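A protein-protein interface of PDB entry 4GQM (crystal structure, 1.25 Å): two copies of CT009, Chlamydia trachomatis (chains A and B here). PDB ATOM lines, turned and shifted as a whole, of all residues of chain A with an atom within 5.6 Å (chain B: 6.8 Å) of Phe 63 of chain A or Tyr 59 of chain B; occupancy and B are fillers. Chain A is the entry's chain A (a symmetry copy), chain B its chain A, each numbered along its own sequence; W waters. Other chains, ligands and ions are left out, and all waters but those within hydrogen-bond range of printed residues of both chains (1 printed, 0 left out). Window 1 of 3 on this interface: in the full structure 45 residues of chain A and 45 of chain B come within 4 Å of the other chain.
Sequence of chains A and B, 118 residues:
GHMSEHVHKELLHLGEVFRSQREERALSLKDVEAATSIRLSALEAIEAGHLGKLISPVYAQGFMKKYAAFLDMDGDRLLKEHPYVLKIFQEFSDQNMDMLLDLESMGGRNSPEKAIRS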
ATOM      1  N   VAL A  58      16.213   6.479  -3.439  1.00  0.00           N
ATOM      2  CA  VAL A  58      15.426   5.238  -3.297  1.00  0.00           C
ATOM      3  C   VAL A  58      14.693   5.422  -1.987  1.00  0.00           C
ATOM      4  O   VAL A  58      15.243   5.162  -0.908  1.00  0.00           O
ATOM      5  CB  VAL A  58      16.298   3.973  -3.309  1.00  0.00           C
ATOM      6  CG1 VAL A  58      15.417   2.757  -3.216  1.00  0.00           C
ATOM      7  CG2 VAL A  58      17.139   3.967  -4.563  1.00  0.00           C
ATOM      8  N   TYR A  59      13.491   5.964  -2.060  1.00  0.00           N
ATOM      9  CA  TYR A  59      12.835   6.438  -0.853  1.00  0.00           C
ATOM     10  C   TYR A  59      12.656   5.311   0.177  1.00  0.00           C
ATOM     11  O   TYR A  59      12.754   5.558   1.375  1.00  0.00           O
ATOM     12  CB  TYR A  59      11.499   7.117  -1.190  1.00  0.00           C
ATOM     13  CG  TYR A  59      11.663   8.491  -1.827  1.00  0.00           C
ATOM     14  CD1 TYR A  59      11.807   9.616  -1.040  1.00  0.00           C
ATOM     15  CD2 TYR A  59      11.742   8.648  -3.203  1.00  0.00           C
ATOM     16  CE1 TYR A  59      11.979  10.875  -1.595  1.00  0.00           C
ATOM     17  CE2 TYR A  59      11.932   9.917  -3.758  1.00  0.00           C
ATOM     18  CZ  TYR A  59      12.021  11.011  -2.941  1.00  0.00           C
ATOM     19  OH  TYR A  59      12.182  12.277  -3.488  1.00  0.00           O
ATOM     20  N   ALA A  60      12.352   4.107  -0.287  1.00  0.00           N
ATOM     21  CA  ALA A  60      12.149   2.987   0.649  1.00  0.00           C
ATOM     22  C   ALA A  60      13.369   2.694   1.476  1.00  0.00           C
ATOM     23  O   ALA A  60      13.256   2.283   2.635  1.00  0.00           O
ATOM     24  CB  ALA A  60      11.788   1.760  -0.134  1.00  0.00           C
ATOM     25  N   GLN A  61      14.552   2.857   0.897  1.00  0.00           N
ATOM     26  CA  GLN A  61      15.817   2.637   1.601  1.00  0.00           C
ATOM     27  C   GLN A  61      15.900   3.615   2.756  1.00  0.00           C
ATOM     28  O   GLN A  61      16.263   3.265   3.882  1.00  0.00           O
ATOM     29  CB  GLN A  61      17.006   2.813   0.625  1.00  0.00           C
ATOM     30  CG  GLN A  61      18.426   2.784   1.262  1.00  0.00           C
ATOM     31  CD  GLN A  61      19.559   3.179   0.279  1.00  0.00           C
ATOM     32  OE1 GLN A  61      19.349   3.729  -0.816  1.00  0.00           O
ATOM     33  NE2 GLN A  61      20.765   2.914   0.704  1.00  0.00           N
ATOM     34  N   GLY A  62      15.572   4.868   2.480  1.00  0.00           N
ATOM     35  CA  GLY A  62      15.621   5.909   3.493  1.00  0.00           C
ATOM     36  C   GLY A  62      14.588   5.626   4.563  1.00  0.00           C
ATOM     37  O   GLY A  62      14.865   5.820   5.762  1.00  0.00           O
ATOM     38  N   PHE A  63      13.381   5.190   4.201  1.00  0.00           N
ATOM     39  CA  PHE A  63      12.379   4.893   5.213  1.00  0.00           C
ATOM     40  C   PHE A  63      12.896   3.796   6.145  1.00  0.00           C
ATOM     41  O   PHE A  63      12.710   3.849   7.359  1.00  0.00           O
ATOM     42  CB  PHE A  63      11.064   4.390   4.591  1.00  0.00           C
ATOM     43  CG  PHE A  63      10.375   5.349   3.631  1.00  0.00           C
ATOM     44  CD1 PHE A  63      10.466   6.723   3.774  1.00  0.00           C
ATOM     45  CD2 PHE A  63       9.608   4.842   2.577  1.00  0.00           C
ATOM     46  CE1 PHE A  63       9.812   7.569   2.833  1.00  0.00           C
ATOM     47  CE2 PHE A  63       8.961   5.693   1.666  1.00  0.00           C
ATOM     48  CZ  PHE A  63       9.044   7.018   1.826  1.00  0.00           C
ATOM     49  N   MET A  64      13.497   2.760   5.561  1.00  0.00           N
ATOM     50  CA  MET A  64      14.017   1.671   6.374  1.00  0.00           C
ATOM     51  C   MET A  64      15.103   2.145   7.345  1.00  0.00           C
ATOM     52  O   MET A  64      15.123   1.742   8.512  1.00  0.00           O
ATOM     53  CB  MET A  64      14.538   0.541   5.505  1.00  0.00           C
ATOM     54  CG  MET A  64      13.421  -0.232   4.835  1.00  0.00           C
ATOM     55  SD  MET A  64      14.139  -1.537   3.818  1.00  0.00           S
ATOM     56  CE  MET A  64      12.656  -2.373   3.257  1.00  0.00           C
ATOM     57  N   LYS A  65      16.023   2.964   6.873  1.00  0.00           N
ATOM     58  CA  LYS A  65      17.093   3.509   7.707  1.00  0.00           C
ATOM     59  C   LYS A  65      16.548   4.312   8.853  1.00  0.00           C
ATOM     60  O   LYS A  65      17.003   4.212   9.988  1.00  0.00           O
ATOM     61  CB  LYS A  65      17.980   4.440   6.897  1.00  0.00           C
ATOM     62  CG  LYS A  65      18.836   3.751   5.916  1.00  0.00           C
ATOM     63  CD  LYS A  65      19.703   4.736   5.195  1.00  0.00           C
ATOM     64  CE  LYS A  65      20.762   4.016   4.435  1.00  0.00           C
ATOM     65  NZ  LYS A  65      21.458   4.955   3.563  1.00  0.00           N
ATOM     66  N   LYS A  66      15.572   5.165   8.553  1.00  0.00           N
ATOM     67  CA  LYS A  66      14.999   6.047   9.576  1.00  0.00           C
ATOM     68  C   LYS A  66      14.206   5.238  10.608  1.00  0.00           C
ATOM     69  O   LYS A  66      14.257   5.518  11.812  1.00  0.00           O
ATOM     70  CB  LYS A  66      14.093   7.115   8.939  1.00  0.00           C
ATOM     71  CG  LYS A  66      14.809   8.229   8.186  1.00  0.00           C
ATOM     72  CD  LYS A  66      13.824   9.250   7.613  1.00  0.00           C
ATOM     73  N   TYR A  67      13.474   4.235  10.140  1.00  0.00           N
ATOM     74  CA  TYR A  67      12.708   3.397  11.052  1.00  0.00           C
ATOM     75  C   TYR A  67      13.683   2.621  11.948  1.00  0.00           C
ATOM     76  O   TYR A  67      13.509   2.534  13.166  1.00  0.00           O
ATOM     77  CB  TYR A  67      11.818   2.474  10.220  1.00  0.00           C
ATOM     78  CG  TYR A  67      10.783   1.651  10.959  1.00  0.00           C
ATOM     79  CD1 TYR A  67      10.516   1.841  12.297  1.00  0.00           C
ATOM     80  CD2 TYR A  67      10.057   0.693  10.298  1.00  0.00           C
ATOM     81  CE1 TYR A  67       9.541   1.094  12.939  1.00  0.00           C
ATOM     82  CE2 TYR A  67       9.078  -0.057  10.937  1.00  0.00           C
ATOM     83  CZ  TYR A  67       8.836   0.139  12.271  1.00  0.00           C
ATOM     84  OH  TYR A  67       7.877  -0.566  12.959  1.00  0.00           O
ATOM     85  N   ALA A  68      14.747   2.084  11.351  1.00  0.00           N
ATOM     86  CA  ALA A  68      15.725   1.340  12.135  1.00  0.00           C
ATOM     87  C   ALA A  68      16.319   2.232  13.206  1.00  0.00           C
ATOM     88  O   ALA A  68      16.483   1.797  14.357  1.00  0.00           O
ATOM     89  CB  ALA A  68      16.789   0.793  11.242  1.00  0.00           C
ATOM     90  N   PHE B  18      11.687  -5.557  11.912  1.00  0.00           N
ATOM     91  CA  PHE B  18      11.081  -4.282  12.296  1.00  0.00           C
ATOM     92  C   PHE B  18       9.877  -4.499  13.205  1.00  0.00           C
ATOM     93  O   PHE B  18       9.778  -3.894  14.270  1.00  0.00           O
ATOM     94  CB  PHE B  18      10.682  -3.465  11.058  1.00  0.00           C
ATOM     95  CG  PHE B  18      11.825  -2.808  10.367  1.00  0.00           C
ATOM     96  CD1 PHE B  18      12.380  -1.655  10.883  1.00  0.00           C
ATOM     97  CD2 PHE B  18      12.280  -3.239   9.148  1.00  0.00           C
ATOM     98  CE1 PHE B  18      13.394  -1.018  10.217  1.00  0.00           C
ATOM     99  CE2 PHE B  18      13.329  -2.568   8.485  1.00  0.00           C
ATOM    100  CZ  PHE B  18      13.881  -1.489   9.033  1.00  0.00           C
ATOM    101  N   SER B  37       7.663  10.666  11.442  1.00  0.00           N
ATOM    102  CA  SER B  37       7.029  11.293  10.287  1.00  0.00           C
ATOM    103  C   SER B  37       7.137  10.462   9.003  1.00  0.00           C
ATOM    104  O   SER B  37       6.973  10.998   7.897  1.00  0.00           O
ATOM    105  CB  SER B  37       7.581  12.703  10.063  1.00  0.00           C
ATOM    106  OG  SER B  37       7.222  13.533  11.150  1.00  0.00           O
ATOM    107  N   ILE B  38       7.448   9.176   9.131  1.00  0.00           N
ATOM    108  CA  ILE B  38       7.385   8.270   8.002  1.00  0.00           C
ATOM    109  C   ILE B  38       5.923   7.892   7.833  1.00  0.00           C
ATOM    110  O   ILE B  38       5.235   7.484   8.780  1.00  0.00           O
ATOM    111  CB  ILE B  38       8.186   6.979   8.258  1.00  0.00           C
ATOM    112  CG1 ILE B  38       9.648   7.304   8.530  1.00  0.00           C
ATOM    113  CG2 ILE B  38       8.056   6.051   7.085  1.00  0.00           C
ATOM    114  CD1 ILE B  38      10.375   6.120   9.125  1.00  0.00           C
ATOM    115  N   ARG B  39       5.413   8.024   6.628  1.00  0.00           N
ATOM    116  CA  ARG B  39       4.014   7.719   6.404  1.00  0.00           C
ATOM    117  C   ARG B  39       3.628   6.312   6.805  1.00  0.00           C
ATOM    118  O   ARG B  39       4.353   5.334   6.545  1.00  0.00           O
ATOM    119  CB  ARG B  39       3.712   7.864   4.925  1.00  0.00           C
ATOM    120  CG  ARG B  39       3.831   9.223   4.390  1.00  0.00           C
ATOM    121  CD  ARG B  39       2.709  10.057   4.830  1.00  0.00           C
ATOM    122  NE  ARG B  39       2.905  11.397   4.316  1.00  0.00           N
ATOM    123  CZ  ARG B  39       2.187  12.440   4.700  1.00  0.00           C
ATOM    124  NH1 ARG B  39       1.221  12.282   5.606  1.00  0.00           N
ATOM    125  NH2 ARG B  39       2.436  13.631   4.191  1.00  0.00           N
ATOM    126  N   ALA B  42       3.983   3.538   4.220  1.00  0.00           N
ATOM    127  CA  ALA B  42       5.359   3.092   4.017  1.00  0.00           C
ATOM    128  C   ALA B  42       5.799   2.126   5.131  1.00  0.00           C
ATOM    129  O   ALA B  42       6.420   1.098   4.876  1.00  0.00           O
ATOM    130  CB  ALA B  42       6.279   4.281   3.924  1.00  0.00           C
ATOM    131  N   LEU B  43       5.446   2.441   6.375  1.00  0.00           N
ATOM    132  CA  LEU B  43       5.750   1.561   7.489  1.00  0.00           C
ATOM    133  C   LEU B  43       5.065   0.212   7.297  1.00  0.00           C
ATOM    134  O   LEU B  43       5.673  -0.832   7.584  1.00  0.00           O
ATOM    135  CB  LEU B  43       5.318   2.211   8.814  1.00  0.00           C
ATOM    136  CG  LEU B  43       6.061   3.488   9.180  1.00  0.00           C
ATOM    137  CD1 LEU B  43       5.388   4.177  10.337  1.00  0.00           C
ATOM    138  CD2 LEU B  43       7.548   3.221   9.482  1.00  0.00           C
ATOM    139  N   ALA B  45       4.210  -1.196   4.505  1.00  0.00           N
ATOM    140  CA  ALA B  45       4.844  -1.903   3.401  1.00  0.00           C
ATOM    141  C   ALA B  45       6.190  -2.504   3.831  1.00  0.00           C
ATOM    142  O   ALA B  45       6.550  -3.597   3.382  1.00  0.00           O
ATOM    143  CB  ALA B  45       5.024  -0.955   2.211  1.00  0.00           C
ATOM    144  N   ILE B  46       6.933  -1.781   4.655  1.00  0.00           N
ATOM    145  CA  ILE B  46       8.172  -2.311   5.211  1.00  0.00           C
ATOM    146  C   ILE B  46       7.873  -3.565   6.033  1.00  0.00           C
ATOM    147  O   ILE B  46       8.506  -4.613   5.847  1.00  0.00           O
ATOM    148  CB  ILE B  46       8.888  -1.266   6.069  1.00  0.00           C
ATOM    149  CG1 ILE B  46       9.449  -0.154   5.189  1.00  0.00           C
ATOM    150  CG2 ILE B  46      10.010  -1.924   6.905  1.00  0.00           C
ATOM    151  CD1 ILE B  46       9.909   1.043   5.966  1.00  0.00           C
ATOM    152  N   GLY B  52       6.546  -4.051  -4.251  1.00  0.00           N
ATOM    153  CA  GLY B  52       5.767  -3.179  -5.112  1.00  0.00           C
ATOM    154  C   GLY B  52       5.285  -1.952  -4.386  1.00  0.00           C
ATOM    155  O   GLY B  52       5.331  -0.835  -4.944  1.00  0.00           O
ATOM    156  N   LYS B  53       4.775  -2.092  -3.177  1.00  0.00           N
ATOM    157  CA  LYS B  53       4.306  -0.924  -2.453  1.00  0.00           C
ATOM    158  C   LYS B  53       5.432   0.019  -2.112  1.00  0.00           C
ATOM    159  O   LYS B  53       5.195   1.218  -1.936  1.00  0.00           O
ATOM    160  CB  LYS B  53       3.528  -1.337  -1.188  1.00  0.00           C
ATOM    161  CG  LYS B  53       2.189  -1.925  -1.478  1.00  0.00           C
ATOM    162  CD  LYS B  53       1.529  -2.504  -0.223  1.00  0.00           C
ATOM    163  CE  LYS B  53       0.276  -3.272  -0.631  1.00  0.00           C
ATOM    164  NZ  LYS B  53      -0.468  -3.847   0.480  1.00  0.00           N
ATOM    165  N   LEU B  54       6.650  -0.505  -1.955  1.00  0.00           N
ATOM    166  CA  LEU B  54       7.809   0.325  -1.640  1.00  0.00           C
ATOM    167  C   LEU B  54       8.397   1.066  -2.826  1.00  0.00           C
ATOM    168  O   LEU B  54       8.847   2.197  -2.687  1.00  0.00           O
ATOM    169  CB  LEU B  54       8.875  -0.565  -0.994  1.00  0.00           C
ATOM    170  CG  LEU B  54       8.558  -1.129   0.384  1.00  0.00           C
ATOM    171  CD1 LEU B  54       9.551  -2.211   0.816  1.00  0.00           C
ATOM    172  CD2 LEU B  54       8.503  -0.025   1.416  1.00  0.00           C
ATOM    173  N   ILE B  55       8.453   0.407  -3.980  1.00  0.00           N
ATOM    174  CA  ILE B  55       9.150   0.906  -5.179  1.00  0.00           C
ATOM    175  C   ILE B  55       8.258   1.556  -6.222  1.00  0.00           C
ATOM    176  O   ILE B  55       8.719   2.369  -7.005  1.00  0.00           O
ATOM    177  CB  ILE B  55       9.863  -0.262  -5.891  1.00  0.00           C
ATOM    178  CG1 ILE B  55      10.983  -0.839  -5.029  1.00  0.00           C
ATOM    179  CG2 ILE B  55      10.407   0.173  -7.260  1.00  0.00           C
ATOM    180  CD1 ILE B  55      12.103   0.172  -4.726  1.00  0.00           C
ATOM    181  N   SER B  56       6.996   1.164  -6.260  1.00  0.00           N
ATOM    182  CA  SER B  56       6.121   1.644  -7.352  1.00  0.00           C
ATOM    183  C   SER B  56       5.812   3.137  -7.342  1.00  0.00           C
ATOM    184  O   SER B  56       5.717   3.730  -8.428  1.00  0.00           O
ATOM    185  CB  SER B  56       4.771   0.879  -7.338  1.00  0.00           C
ATOM    186  OG  SER B  56       4.967  -0.461  -7.619  1.00  0.00           O
ATOM    187  N   PRO B  57       5.590   3.774  -6.207  1.00  0.00           N
ATOM    188  CA  PRO B  57       5.193   5.199  -6.264  1.00  0.00           C
ATOM    189  C   PRO B  57       6.219   6.099  -6.864  1.00  0.00           C
ATOM    190  O   PRO B  57       7.424   5.934  -6.669  1.00  0.00           O
ATOM    191  CB  PRO B  57       4.996   5.563  -4.772  1.00  0.00           C
ATOM    192  CG  PRO B  57       4.656   4.278  -4.114  1.00  0.00           C
ATOM    193  CD  PRO B  57       5.531   3.229  -4.825  1.00  0.00           C
ATOM    194  N   VAL B  58       5.754   7.127  -7.584  1.00  0.00           N
ATOM    195  CA  VAL B  58       6.621   8.266  -7.944  1.00  0.00           C
ATOM    196  C   VAL B  58       6.449   9.230  -6.790  1.00  0.00           C
ATOM    197  O   VAL B  58       5.488  10.011  -6.751  1.00  0.00           O
ATOM    198  CB  VAL B  58       6.249   8.897  -9.295  1.00  0.00           C
ATOM    199  CG1 VAL B  58       7.212  10.009  -9.609  1.00  0.00           C
ATOM    200  CG2 VAL B  58       6.260   7.824 -10.356  1.00  0.00           C
ATOM    201  N   TYR B  59       7.313   9.116  -5.799  1.00  0.00           N
ATOM    202  CA  TYR B  59       7.062   9.792  -4.537  1.00  0.00           C
ATOM    203  C   TYR B  59       6.931  11.312  -4.723  1.00  0.00           C
ATOM    204  O   TYR B  59       6.139  11.945  -4.031  1.00  0.00           O
ATOM    205  CB  TYR B  59       8.143   9.437  -3.504  1.00  0.00           C
ATOM    206  CG  TYR B  59       8.010   8.024  -2.952  1.00  0.00           C
ATOM    207  CD1 TYR B  59       7.182   7.766  -1.878  1.00  0.00           C
ATOM    208  CD2 TYR B  59       8.655   6.949  -3.546  1.00  0.00           C
ATOM    209  CE1 TYR B  59       7.027   6.485  -1.369  1.00  0.00           C
ATOM    210  CE2 TYR B  59       8.483   5.657  -3.040  1.00  0.00           C
ATOM    211  CZ  TYR B  59       7.690   5.454  -1.944  1.00  0.00           C
ATOM    212  OH  TYR B  59       7.538   4.178  -1.420  1.00  0.00           O
ATOM    213  N   ALA B  60       7.732  11.887  -5.610  1.00  0.00           N
ATOM    214  CA  ALA B  60       7.669  13.344  -5.822  1.00  0.00           C
ATOM    215  C   ALA B  60       6.317  13.804  -6.291  1.00  0.00           C
ATOM    216  O   ALA B  60       5.882  14.910  -5.958  1.00  0.00           O
ATOM    217  CB  ALA B  60       8.693  13.729  -6.847  1.00  0.00           C
ATOM    218  N   GLN B  61       5.644  12.995  -7.099  1.00  0.00           N
ATOM    219  CA  GLN B  61       4.304  13.309  -7.600  1.00  0.00           C
ATOM    220  C   GLN B  61       3.362  13.420  -6.418  1.00  0.00           C
ATOM    221  O   GLN B  61       2.549  14.342  -6.318  1.00  0.00           O
ATOM    222  CB  GLN B  61       3.839  12.216  -8.594  1.00  0.00           C
ATOM    223  CG  GLN B  61       2.364  12.315  -9.080  1.00  0.00           C
ATOM    224  CD  GLN B  61       1.891  11.083  -9.894  1.00  0.00           C
ATOM    225  OE1 GLN B  61       2.515  10.007  -9.926  1.00  0.00           O
ATOM    226  NE2 GLN B  61       0.762  11.250 -10.529  1.00  0.00           N
ATOM    227  N   GLY B  62       3.458  12.462  -5.509  1.00  0.00           N
ATOM    228  CA  GLY B  62       2.605  12.441  -4.333  1.00  0.00           C
ATOM    229  C   GLY B  62       2.921  13.632  -3.454  1.00  0.00           C
ATOM    230  O   GLY B  62       1.999  14.256  -2.895  1.00  0.00           O
ATOM    231  N   PHE B  63       4.195  13.984  -3.271  1.00  0.00           N
ATOM    232  CA  PHE B  63       4.522  15.137  -2.446  1.00  0.00           C
ATOM    233  C   PHE B  63       3.879  16.393  -3.037  1.00  0.00           C
ATOM    234  O   PHE B  63       3.355  17.241  -2.317  1.00  0.00           O
ATOM    235  CB  PHE B  63       6.040  15.382  -2.376  1.00  0.00           C
ATOM    236  CG  PHE B  63       6.870  14.245  -1.800  1.00  0.00           C
ATOM    237  CD1 PHE B  63       6.371  13.387  -0.835  1.00  0.00           C
ATOM    238  CD2 PHE B  63       8.185  14.056  -2.239  1.00  0.00           C
ATOM    239  CE1 PHE B  63       7.192  12.330  -0.348  1.00  0.00           C
ATOM    240  CE2 PHE B  63       8.982  13.014  -1.738  1.00  0.00           C
ATOM    241  CZ  PHE B  63       8.494  12.204  -0.793  1.00  0.00           C
ATOM    242  N   MET B  64       3.978  16.542  -4.357  1.00  0.00           N
ATOM    243  CA  MET B  64       3.396  17.710  -5.001  1.00  0.00           C
ATOM    244  C   MET B  64       1.878  17.782  -4.799  1.00  0.00           C
ATOM    245  O   MET B  64       1.330  18.855  -4.528  1.00  0.00           O
ATOM    246  CB  MET B  64       3.737  17.746  -6.479  1.00  0.00           C
ATOM    247  CG  MET B  64       5.190  18.092  -6.726  1.00  0.00           C
ATOM    248  SD  MET B  64       5.499  18.096  -8.503  1.00  0.00           S
ATOM    249  CE  MET B  64       7.203  18.652  -8.542  1.00  0.00           C
ATOM    250  N   ASN B  96       9.038   2.073 -13.079  1.00  0.00           N
ATOM    251  CA  ASN B  96       9.009   1.347 -11.819  1.00  0.00           C
ATOM    252  C   ASN B  96       8.291   0.006 -12.007  1.00  0.00           C
ATOM    253  O   ASN B  96       8.749  -1.035 -11.528  1.00  0.00           O
ATOM    254  CB  ASN B  96       8.283   2.160 -10.760  1.00  0.00           C
ATOM    255  CG  ASN B  96       9.024   3.424 -10.351  1.00  0.00           C
ATOM    256  OD1 ASN B  96      10.221   3.587 -10.601  1.00  0.00           O
ATOM    257  ND2 ASN B  96       8.307   4.325  -9.671  1.00  0.00           N
HETATM  258  O   HOH W   1      11.562   3.370  -2.882  1.00  0.00           O
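The side-chain hydroxyl (OH) of Tyr 59 of chain B sits at hydrogen-bond distance from the backbone carbonyl oxygen (O) of Leu 54 of chain B (2.7 Å).
Tyr 59 of chain A touches Tyr 59 of chain B.
CB of Ala 60 of chain A touches CB of Leu 54 of chain B, 3.8 Å away.
O of Phe 63 of chain A touches CD1 of Ile 38 of chain B (3.7 Å).
Phe 63 of chain A touches Ala 42 of chain B (CD2 to CB, 3.6 Å).
Phe 63 of chain A touches Ile 46 of chain B.
Phe 18 of chain B touches Met 64 of chain A.
Met 64 of chain A touches Ile 46 of chain B (CG to CD1, 3.9 Å).
Leu 54 of chain B touches Met 64 of chain A (CD1 to CE, 3.95 Å).
Phe 18 of chain B touches Tyr 67 of chain A (CD1 to CD2, 3.4 Å).
Tyr 67 of chain A touches Ile 38 of chain B (N to CD1, 3.8 Å).
Printed residues of chain B within 4 Å of Tyr 59 of chain A: Tyr 59 and Phe 63.
Printed residues of chain B within 4 Å of Ala 60 of chain A: Leu 54.
Phe 63 of chain A touches four residues of chain B.
Printed residues of chain A within 4 Å of Phe 18 of chain B: Met 64 (3.5 Å), Tyr 67 (3.4 Å) and Ala 68 (3.6 Å).
Of the printed residues of chain A, Leu 43 of chain B touches Tyr 67.
Tyr 59 of chain B touches just these residues of chain A: Tyr 59 and Phe 63.
The nearest residue of chain B that does not touch Phe 63 of chain A is Leu 54 of chain B (5.1 Å).
Of the 22 printed residues of chain B, 8 touch a printed residue of chain A.
Printed residues of chain B that touch a printed residue of chain A: Phe 18, Ile 38, Ala 42, Leu 43, Ile 46, Leu 54, Tyr 59 and Phe 63.
Hydrophobic or aromatic side chains of chain B that line the printed part of chain A: Phe 18, Ile 38, Ala 42, Leu 43, Ile 46, Leu 54, Tyr 59 and Phe 63.
Among the printed residues, 15 pairs touch across the chains.
Among the printed residues, no Asp or Glu carboxylate lies within 4 Å of a Lys or Arg side-chain nitrogen of the other chain.
Tyr 59 of chain A touches its own counterpart, Tyr 59 of chain B.
Tyr 59 of chain A touches Phe 63 of chain B, and with the chains exchanged Phe 63 of chain A touches Tyr 59 of chain B.
Water W1 lies within hydrogen-bond range of N of Ala 60 of chain A, O of Leu 54 of chain B and N of Tyr 59 of chain A.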
